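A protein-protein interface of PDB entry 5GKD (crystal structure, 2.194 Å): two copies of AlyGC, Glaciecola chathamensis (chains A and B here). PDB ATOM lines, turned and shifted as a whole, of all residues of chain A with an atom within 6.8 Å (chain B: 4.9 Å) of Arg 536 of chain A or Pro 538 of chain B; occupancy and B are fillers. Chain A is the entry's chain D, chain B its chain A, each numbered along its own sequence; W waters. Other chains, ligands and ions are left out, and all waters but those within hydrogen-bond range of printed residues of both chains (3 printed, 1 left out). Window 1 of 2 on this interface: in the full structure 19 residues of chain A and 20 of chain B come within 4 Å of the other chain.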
ATOM      1  N   SER A 500      18.241 -27.037 -22.738  1.00  0.00           N
ATOM      2  CA  SER A 500      17.058 -26.256 -23.068  1.00  0.00           C
ATOM      3  C   SER A 500      16.848 -25.105 -22.097  1.00  0.00           C
ATOM      4  O   SER A 500      16.147 -24.160 -22.431  1.00  0.00           O
ATOM      5  CB  SER A 500      15.826 -27.161 -23.111  1.00  0.00           C
ATOM      6  OG  SER A 500      15.781 -27.963 -21.949  1.00  0.00           O
ATOM      7  N   THR A 501      17.461 -25.155 -20.926  1.00  0.00           N
ATOM      8  CA  THR A 501      17.507 -24.041 -19.995  1.00  0.00           C
ATOM      9  C   THR A 501      18.963 -23.723 -19.694  1.00  0.00           C
ATOM     10  O   THR A 501      19.776 -24.632 -19.507  1.00  0.00           O
ATOM     11  CB  THR A 501      16.757 -24.360 -18.691  1.00  0.00           C
ATOM     12  OG1 THR A 501      15.359 -24.334 -18.940  1.00  0.00           O
ATOM     13  CG2 THR A 501      17.054 -23.325 -17.622  1.00  0.00           C
ATOM     14  N   GLU A 504      18.182 -21.455 -14.167  1.00  0.00           N
ATOM     15  CA  GLU A 504      16.957 -21.716 -13.435  1.00  0.00           C
ATOM     16  C   GLU A 504      17.027 -20.996 -12.096  1.00  0.00           C
ATOM     17  O   GLU A 504      17.973 -21.203 -11.335  1.00  0.00           O
ATOM     18  CB  GLU A 504      16.782 -23.219 -13.215  1.00  0.00           C
ATOM     19  CG  GLU A 504      15.603 -23.575 -12.353  1.00  0.00           C
ATOM     20  CD  GLU A 504      15.617 -25.025 -11.925  1.00  0.00           C
ATOM     21  OE1 GLU A 504      14.710 -25.760 -12.334  1.00  0.00           O
ATOM     22  OE2 GLU A 504      16.531 -25.435 -11.176  1.00  0.00           O
ATOM     23  N   ILE A 505      16.016 -20.181 -11.793  1.00  0.00           N
ATOM     24  CA  ILE A 505      15.958 -19.424 -10.543  1.00  0.00           C
ATOM     25  C   ILE A 505      15.112 -20.202  -9.533  1.00  0.00           C
ATOM     26  O   ILE A 505      13.893 -20.308  -9.674  1.00  0.00           O
ATOM     27  CB  ILE A 505      15.400 -18.014 -10.764  1.00  0.00           C
ATOM     28  CG1 ILE A 505      16.271 -17.279 -11.773  1.00  0.00           C
ATOM     29  CG2 ILE A 505      15.334 -17.241  -9.424  1.00  0.00           C
ATOM     30  CD1 ILE A 505      15.729 -15.953 -12.206  1.00  0.00           C
ATOM     31  N   ASN A 506      15.747 -20.736  -8.506  1.00  0.00           N
ATOM     32  CA  ASN A 506      15.063 -21.462  -7.452  1.00  0.00           C
ATOM     33  C   ASN A 506      14.770 -20.522  -6.272  1.00  0.00           C
ATOM     34  O   ASN A 506      15.144 -19.353  -6.285  1.00  0.00           O
ATOM     35  CB  ASN A 506      15.907 -22.658  -7.016  1.00  0.00           C
ATOM     36  CG  ASN A 506      15.747 -23.851  -7.933  1.00  0.00           C
ATOM     37  OD1 ASN A 506      14.692 -24.457  -7.970  1.00  0.00           O
ATOM     38  ND2 ASN A 506      16.802 -24.214  -8.646  1.00  0.00           N
ATOM     39  N   GLY A 528      10.396 -24.826 -27.635  1.00  0.00           N
ATOM     40  CA  GLY A 528      10.081 -24.556 -26.249  1.00  0.00           C
ATOM     41  C   GLY A 528      11.264 -24.410 -25.319  1.00  0.00           C
ATOM     42  O   GLY A 528      11.071 -24.475 -24.114  1.00  0.00           O
ATOM     43  N   ASN A 529      12.480 -24.228 -25.841  1.00  0.00           N
ATOM     44  CA  ASN A 529      13.623 -23.881 -24.999  1.00  0.00           C
ATOM     45  C   ASN A 529      13.345 -22.565 -24.260  1.00  0.00           C
ATOM     46  O   ASN A 529      12.550 -21.734 -24.706  1.00  0.00           O
ATOM     47  CB  ASN A 529      14.911 -23.736 -25.828  1.00  0.00           C
ATOM     48  CG  ASN A 529      15.401 -25.064 -26.459  1.00  0.00           C
ATOM     49  OD1 ASN A 529      15.097 -26.152 -25.996  1.00  0.00           O
ATOM     50  ND2 ASN A 529      16.177 -24.943 -27.525  1.00  0.00           N
ATOM     51  N   THR A 530      14.001 -22.386 -23.111  1.00  0.00           N
ATOM     52  CA  THR A 530      13.811 -21.210 -22.254  1.00  0.00           C
ATOM     53  C   THR A 530      15.171 -20.848 -21.677  1.00  0.00           C
ATOM     54  O   THR A 530      15.711 -21.593 -20.853  1.00  0.00           O
ATOM     55  CB  THR A 530      12.825 -21.477 -21.115  1.00  0.00           C
ATOM     56  OG1 THR A 530      13.267 -22.614 -20.379  1.00  0.00           O
ATOM     57  CG2 THR A 530      11.409 -21.723 -21.615  1.00  0.00           C
ATOM     58  N   ARG A 533      14.630 -18.932 -16.578  1.00  0.00           N
ATOM     59  CA  ARG A 533      13.296 -19.219 -16.089  1.00  0.00           C
ATOM     60  C   ARG A 533      13.386 -19.456 -14.592  1.00  0.00           C
ATOM     61  O   ARG A 533      14.453 -19.771 -14.064  1.00  0.00           O
ATOM     62  CB  ARG A 533      12.690 -20.437 -16.790  1.00  0.00           C
ATOM     63  CG  ARG A 533      13.455 -21.749 -16.559  1.00  0.00           C
ATOM     64  CD  ARG A 533      12.653 -22.977 -17.041  1.00  0.00           C
ATOM     65  NE  ARG A 533      13.433 -24.209 -16.951  1.00  0.00           N
ATOM     66  CZ  ARG A 533      13.522 -24.952 -15.848  1.00  0.00           C
ATOM     67  NH1 ARG A 533      12.871 -24.604 -14.753  1.00  0.00           N
ATOM     68  NH2 ARG A 533      14.252 -26.056 -15.836  1.00  0.00           N
ATOM     69  N   THR A 534      12.258 -19.276 -13.911  1.00  0.00           N
ATOM     70  CA  THR A 534      12.168 -19.817 -12.568  1.00  0.00           C
ATOM     71  C   THR A 534      12.073 -21.332 -12.648  1.00  0.00           C
ATOM     72  O   THR A 534      11.750 -21.911 -13.689  1.00  0.00           O
ATOM     73  CB  THR A 534      10.937 -19.293 -11.822  1.00  0.00           C
ATOM     74  OG1 THR A 534       9.751 -19.771 -12.466  1.00  0.00           O
ATOM     75  CG2 THR A 534      10.906 -17.771 -11.771  1.00  0.00           C
ATOM     76  N   THR A 535      12.317 -21.970 -11.517  1.00  0.00           N
ATOM     77  CA  THR A 535      11.866 -23.334 -11.354  1.00  0.00           C
ATOM     78  C   THR A 535      10.381 -23.426 -11.686  1.00  0.00           C
ATOM     79  O   THR A 535       9.617 -22.465 -11.529  1.00  0.00           O
ATOM     80  CB  THR A 535      12.112 -23.803  -9.927  1.00  0.00           C
ATOM     81  OG1 THR A 535      11.537 -25.097  -9.766  1.00  0.00           O
ATOM     82  CG2 THR A 535      11.457 -22.826  -8.936  1.00  0.00           C
ATOM     83  N   ARG A 536       9.973 -24.582 -12.160  1.00  0.00           N
ATOM     84  CA  ARG A 536       8.566 -24.838 -12.402  1.00  0.00           C
ATOM     85  C   ARG A 536       7.888 -25.496 -11.212  1.00  0.00           C
ATOM     86  O   ARG A 536       6.679 -25.730 -11.258  1.00  0.00           O
ATOM     87  CB  ARG A 536       8.400 -25.695 -13.653  1.00  0.00           C
ATOM     88  CG  ARG A 536       9.003 -25.055 -14.900  1.00  0.00           C
ATOM     89  CD  ARG A 536       8.635 -25.836 -16.146  1.00  0.00           C
ATOM     90  NE  ARG A 536       9.319 -25.360 -17.337  1.00  0.00           N
ATOM     91  CZ  ARG A 536      10.423 -25.892 -17.845  1.00  0.00           C
ATOM     92  NH1 ARG A 536      11.004 -26.928 -17.262  1.00  0.00           N
ATOM     93  NH2 ARG A 536      10.944 -25.380 -18.952  1.00  0.00           N
ATOM     94  N   LEU A 537       8.623 -25.798 -10.164  1.00  0.00           N
ATOM     95  CA  LEU A 537       7.936 -26.172  -8.935  1.00  0.00           C
ATOM     96  C   LEU A 537       7.440 -24.902  -8.238  1.00  0.00           C
ATOM     97  O   LEU A 537       8.154 -23.905  -8.219  1.00  0.00           O
ATOM     98  CB  LEU A 537       8.874 -26.952  -8.013  1.00  0.00           C
ATOM     99  CG  LEU A 537       9.414 -28.342  -8.402  1.00  0.00           C
ATOM    100  CD1 LEU A 537      10.405 -28.301  -9.566  1.00  0.00           C
ATOM    101  CD2 LEU A 537      10.055 -28.998  -7.184  1.00  0.00           C
ATOM    102  N   PRO A 538       6.218 -24.893  -7.701  1.00  0.00           N
ATOM    103  CA  PRO A 538       5.683 -23.668  -7.086  1.00  0.00           C
ATOM    104  C   PRO A 538       6.609 -23.131  -6.008  1.00  0.00           C
ATOM    105  O   PRO A 538       6.998 -23.851  -5.086  1.00  0.00           O
ATOM    106  CB  PRO A 538       4.343 -24.121  -6.495  1.00  0.00           C
ATOM    107  CG  PRO A 538       4.003 -25.354  -7.219  1.00  0.00           C
ATOM    108  CD  PRO A 538       5.280 -26.018  -7.584  1.00  0.00           C
ATOM    109  N   MET A 539       6.960 -21.857  -6.136  1.00  0.00           N
ATOM    110  CA  MET A 539       8.006 -21.269  -5.317  1.00  0.00           C
ATOM    111  C   MET A 539       7.465 -20.837  -3.962  1.00  0.00           C
ATOM    112  O   MET A 539       6.257 -20.668  -3.765  1.00  0.00           O
ATOM    113  CB  MET A 539       8.636 -20.074  -6.028  1.00  0.00           C
ATOM    114  CG  MET A 539       9.374 -20.451  -7.308  1.00  0.00           C
ATOM    115  SD  MET A 539      10.228 -19.088  -8.088  1.00  0.00           S
ATOM    116  CE  MET A 539      11.566 -18.860  -6.932  1.00  0.00           C
ATOM    117  N   ASP A 565      10.888 -17.307 -18.885  1.00  0.00           N
ATOM    118  CA  ASP A 565       9.603 -17.978 -18.700  1.00  0.00           C
ATOM    119  C   ASP A 565       9.293 -18.058 -17.211  1.00  0.00           C
ATOM    120  O   ASP A 565       9.977 -18.768 -16.470  1.00  0.00           O
ATOM    121  CB  ASP A 565       9.624 -19.371 -19.337  1.00  0.00           C
ATOM    122  CG  ASP A 565       8.222 -19.980 -19.493  1.00  0.00           C
ATOM    123  OD1 ASP A 565       7.237 -19.221 -19.590  1.00  0.00           O
ATOM    124  OD2 ASP A 565       8.119 -21.223 -19.530  1.00  0.00           O
ATOM    125  N   ALA A 566       8.269 -17.333 -16.775  1.00  0.00           N
ATOM    126  CA  ALA A 566       7.825 -17.402 -15.386  1.00  0.00           C
ATOM    127  C   ALA A 566       7.090 -18.705 -15.111  1.00  0.00           C
ATOM    128  O   ALA A 566       6.288 -19.157 -15.920  1.00  0.00           O
ATOM    129  CB  ALA A 566       6.899 -16.231 -15.056  1.00  0.00           C
ATOM    130  N   GLY A 567       7.341 -19.293 -13.944  1.00  0.00           N
ATOM    131  CA  GLY A 567       6.562 -20.433 -13.522  1.00  0.00           C
ATOM    132  C   GLY A 567       5.219 -20.032 -12.944  1.00  0.00           C
ATOM    133  O   GLY A 567       4.995 -18.880 -12.556  1.00  0.00           O
ATOM    134  N   ASN A 568       4.314 -21.007 -12.872  1.00  0.00           N
ATOM    135  CA  ASN A 568       3.006 -20.755 -12.278  1.00  0.00           C
ATOM    136  C   ASN A 568       3.143 -20.367 -10.812  1.00  0.00           C
ATOM    137  O   ASN A 568       3.889 -20.990 -10.054  1.00  0.00           O
ATOM    138  CB  ASN A 568       2.105 -21.979 -12.448  1.00  0.00           C
ATOM    139  CG  ASN A 568       1.377 -21.968 -13.804  1.00  0.00           C
ATOM    140  OD1 ASN A 568       0.249 -21.498 -13.898  1.00  0.00           O
ATOM    141  ND2 ASN A 568       2.042 -22.437 -14.858  1.00  0.00           N
ATOM    142  N   PRO B 117      13.056 -35.844 -12.969  1.00  0.00           N
ATOM    143  CA  PRO B 117      11.813 -35.635 -12.205  1.00  0.00           C
ATOM    144  C   PRO B 117      10.700 -34.945 -12.989  1.00  0.00           C
ATOM    145  O   PRO B 117       9.531 -35.128 -12.635  1.00  0.00           O
ATOM    146  CB  PRO B 117      12.256 -34.770 -11.008  1.00  0.00           C
ATOM    147  CG  PRO B 117      13.709 -34.791 -10.989  1.00  0.00           C
ATOM    148  CD  PRO B 117      14.231 -35.252 -12.321  1.00  0.00           C
ATOM    149  N   GLU B 118      11.005 -34.143 -14.008  1.00  0.00           N
ATOM    150  CA  GLU B 118       9.984 -33.467 -14.811  1.00  0.00           C
ATOM    151  C   GLU B 118       9.851 -34.149 -16.160  1.00  0.00           C
ATOM    152  O   GLU B 118      10.846 -34.293 -16.873  1.00  0.00           O
ATOM    153  CB  GLU B 118      10.313 -31.986 -15.040  1.00  0.00           C
ATOM    154  CG  GLU B 118      10.309 -31.128 -13.807  1.00  0.00           C
ATOM    155  CD  GLU B 118      10.514 -29.654 -14.121  1.00  0.00           C
ATOM    156  OE1 GLU B 118       9.721 -29.083 -14.901  1.00  0.00           O
ATOM    157  OE2 GLU B 118      11.494 -29.078 -13.596  1.00  0.00           O
ATOM    158  N   GLU B 121      11.350 -32.081 -19.071  1.00  0.00           N
ATOM    159  CA  GLU B 121      12.770 -31.780 -19.069  1.00  0.00           C
ATOM    160  C   GLU B 121      13.439 -32.942 -19.793  1.00  0.00           C
ATOM    161  O   GLU B 121      13.533 -34.047 -19.250  1.00  0.00           O
ATOM    162  CB  GLU B 121      13.280 -31.598 -17.647  1.00  0.00           C
ATOM    163  CG  GLU B 121      14.586 -30.849 -17.530  1.00  0.00           C
ATOM    164  CD  GLU B 121      14.512 -29.411 -18.027  1.00  0.00           C
ATOM    165  OE1 GLU B 121      15.490 -28.955 -18.644  1.00  0.00           O
ATOM    166  OE2 GLU B 121      13.482 -28.745 -17.827  1.00  0.00           O
ATOM    167  N   ARG B 536       0.800 -29.977  -7.688  1.00  0.00           N
ATOM    168  CA  ARG B 536       1.166 -28.870  -8.547  1.00  0.00           C
ATOM    169  C   ARG B 536       2.660 -28.833  -8.840  1.00  0.00           C
ATOM    170  O   ARG B 536       3.109 -28.012  -9.650  1.00  0.00           O
ATOM    171  CB  ARG B 536       0.690 -27.559  -7.929  1.00  0.00           C
ATOM    172  CG  ARG B 536      -0.828 -27.534  -7.699  1.00  0.00           C
ATOM    173  CD  ARG B 536      -1.269 -26.177  -7.241  1.00  0.00           C
ATOM    174  NE  ARG B 536      -2.706 -26.059  -7.039  1.00  0.00           N
ATOM    175  CZ  ARG B 536      -3.287 -26.058  -5.844  1.00  0.00           C
ATOM    176  NH1 ARG B 536      -2.556 -26.203  -4.755  1.00  0.00           N
ATOM    177  NH2 ARG B 536      -4.598 -25.920  -5.741  1.00  0.00           N
ATOM    178  N   LEU B 537       3.425 -29.693  -8.211  1.00  0.00           N
ATOM    179  CA  LEU B 537       4.791 -29.911  -8.647  1.00  0.00           C
ATOM    180  C   LEU B 537       4.746 -30.699  -9.948  1.00  0.00           C
ATOM    181  O   LEU B 537       3.965 -31.652 -10.048  1.00  0.00           O
ATOM    182  CB  LEU B 537       5.584 -30.654  -7.582  1.00  0.00           C
ATOM    183  CG  LEU B 537       6.062 -29.809  -6.393  1.00  0.00           C
ATOM    184  CD1 LEU B 537       4.917 -29.321  -5.511  1.00  0.00           C
ATOM    185  CD2 LEU B 537       7.068 -30.592  -5.550  1.00  0.00           C
ATOM    186  N   PRO B 538       5.491 -30.299 -10.983  1.00  0.00           N
ATOM    187  CA  PRO B 538       5.503 -31.074 -12.229  1.00  0.00           C
ATOM    188  C   PRO B 538       5.817 -32.525 -11.917  1.00  0.00           C
ATOM    189  O   PRO B 538       6.755 -32.829 -11.174  1.00  0.00           O
ATOM    190  CB  PRO B 538       6.616 -30.418 -13.059  1.00  0.00           C
ATOM    191  CG  PRO B 538       6.837 -29.089 -12.464  1.00  0.00           C
ATOM    192  CD  PRO B 538       6.494 -29.224 -10.995  1.00  0.00           C
ATOM    193  N   MET B 539       4.994 -33.417 -12.440  1.00  0.00           N
ATOM    194  CA  MET B 539       5.104 -34.826 -12.095  1.00  0.00           C
ATOM    195  C   MET B 539       6.110 -35.540 -12.984  1.00  0.00           C
ATOM    196  O   MET B 539       6.422 -35.107 -14.092  1.00  0.00           O
ATOM    197  CB  MET B 539       3.746 -35.518 -12.194  1.00  0.00           C
ATOM    198  CG  MET B 539       2.688 -34.918 -11.294  1.00  0.00           C
ATOM    199  SD  MET B 539       1.093 -35.737 -11.429  1.00  0.00           S
ATOM    200  CE  MET B 539       1.461 -37.338 -10.749  1.00  0.00           C
ATOM    201  N   GLN B 540       6.606 -36.663 -12.477  1.00  0.00           N
ATOM    202  CA  GLN B 540       7.568 -37.512 -13.163  1.00  0.00           C
ATOM    203  C   GLN B 540       6.908 -38.640 -13.931  1.00  0.00           C
ATOM    204  O   GLN B 540       7.545 -39.244 -14.791  1.00  0.00           O
ATOM    205  CB  GLN B 540       8.542 -38.106 -12.134  1.00  0.00           C
ATOM    206  CG  GLN B 540       9.715 -38.857 -12.726  1.00  0.00           C
ATOM    207  CD  GLN B 540      10.414 -39.744 -11.719  1.00  0.00           C
ATOM    208  OE1 GLN B 540       9.787 -40.606 -11.105  1.00  0.00           O
ATOM    209  NE2 GLN B 540      11.723 -39.549 -11.551  1.00  0.00           N
ATOM    210  N   ASN B 568      -0.117 -28.585 -14.388  1.00  0.00           N
ATOM    211  CA  ASN B 568       0.631 -28.356 -15.620  1.00  0.00           C
ATOM    212  C   ASN B 568       1.587 -29.515 -15.893  1.00  0.00           C
ATOM    213  O   ASN B 568       2.276 -29.997 -14.994  1.00  0.00           O
ATOM    214  CB  ASN B 568       1.394 -27.031 -15.533  1.00  0.00           C
ATOM    215  CG  ASN B 568       0.494 -25.822 -15.776  1.00  0.00           C
ATOM    216  OD1 ASN B 568       0.336 -25.379 -16.911  1.00  0.00           O
ATOM    217  ND2 ASN B 568      -0.094 -25.291 -14.717  1.00  0.00           N
HETATM  218  O   HOH W   1       0.577 -22.618 -17.631  1.00  0.00           O
HETATM  219  O   HOH W   2      14.645 -26.533 -20.148  1.00  0.00           O
HETATM  220  O   HOH W   3      11.731 -26.678 -12.791  1.00  0.00           O
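The side-chain carboxylate of Glu 121 of chain B sits at hydrogen-bond distance from the side-chain hydroxyl of Ser 500 of chain A (3.5 Å). The guanidinium group (NH1) of Arg 536 of chain A is in salt-bridge range of the side-chain carboxylate (OE1) of Glu 118 of chain B. The side-chain carboxylate of Glu 121 of chain B lies within salt-bridge range of the guanidinium group of Arg 533 of chain A (3.4 Å). OE2 of Glu 121 of chain B is in salt-bridge range of NH1 of Arg 536 of chain A (3.1 Å).
OE1 of Glu 504 of chain A is in salt-bridge range of NH1 of Arg 533 of chain A (3.3 Å). The side-chain hydroxyl (OG1) of Thr 535 of chain A lies within hydrogen-bond range of the backbone NH (N) of Leu 537 of chain A, 3.0 Å away. O of Ser 500 of chain A is in hydrogen-bond range of N of Thr 530 of chain A, 2.9 Å away. The guanidinium group of Arg 533 of chain A sits at hydrogen-bond distance from the side-chain hydroxyl of Thr 501 of chain A. The backbone NH (N) of Ile 505 of chain A lies within hydrogen-bond range of the backbone carbonyl oxygen (O) of Arg 533 of chain A (2.8 Å).
Arg 536 of chain A touches Pro 538 of chain B. Leu 537 of chain B touches Leu 537 of chain A (CD2 to CD2, 3.8 Å). CA of Leu 537 of chain A touches CD of Pro 538 of chain B (3.95 Å). Pro 538 of chain A touches Arg 536 of chain B (CD to O, 3.6 Å). Leu 537 of chain B touches Pro 538 of chain A (CD1 to CD, 3.9 Å). Asn 568 of chain A touches Asn 568 of chain B (ND2 to ND2, 3.6 Å).
Glu 504 of chain A touches none of the printed residues of chain B. Asn 506 of chain A touches none of the printed residues of chain B. Printed residues of chain B within 4 Å of Arg 533 of chain A: Glu 121 (3.4 Å). Printed residues of chain B within 4 Å of Leu 537 of chain A: Leu 537 (3.8 Å) and Pro 538 (3.95 Å). Of the printed residues of chain A, Glu 118 of chain B touches Arg 536 (3.4 Å). Printed residues of chain A within 4 Å of Arg 536 of chain B: Pro 538. Of chain A, only Arg 536 and Leu 537 come within 4 Å of Pro 538 of chain B. Of the printed residues of chain A, Asn 568 of chain B touches Asn 568. The nearest residue of chain B that does not touch Arg 536 of chain A is Arg 536 of chain B (4.5 Å). The nearest residue of chain A that does not touch Pro 538 of chain B is Pro 538 of chain A (4.8 Å). The nearest printed residue of chain A that does not touch Asn 568 of chain B is Arg 536 of chain A (6.9 Å).
Hydrophobic or aromatic side chains of chain B that line the printed part of chain A: Leu 537 and Pro 538. Of the 19 printed residues of chain A, 6 touch a printed residue of chain B. Hydrophobic or aromatic side chains of chain A that line the printed part of chain B: Leu 537 and Pro 538.
Arg 536 of chain A touches Pro 538 of chain B, and with the chains exchanged Pro 538 of chain A touches Arg 536 of chain B. Leu 537 of chain B touches its own counterpart, Leu 537 of chain A. Leu 537 of chain A touches Pro 538 of chain B, and with the chains exchanged Pro 538 of chain A touches Leu 537 of chain B. Asn 568 of chain A touches its own counterpart, Asn 568 of chain B. Positions printed for both chains: 536, 537, 538, 539 and 568. Of the 10 pairs that touch across the chains among the printed residues, 6 have their exchanged pair printed and touching as well.
Water W3 lies within hydrogen-bond range of OE2 of Glu 118 of chain B (2.5 Å), N of Arg 536 of chain A (2.8 Å), NH1 of Arg 533 of chain A (3.1 Å), OE1 of Glu 504 of chain A (3.2 Å) and OG1 of Thr 535 of chain A (3.4 Å). Water W2 lies within hydrogen-bond range of OG of Ser 500 of chain A (2.6 Å), OG1 of Thr 501 of chain A (2.6 Å) and OE1 of Glu 121 of chain B (3.0 Å). Water W1 lies within hydrogen-bond range of the side-chain amide oxygen (OD1) of Asn 568 of chain B and the side-chain amide nitrogen (ND2) of Asn 568 of chain A.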
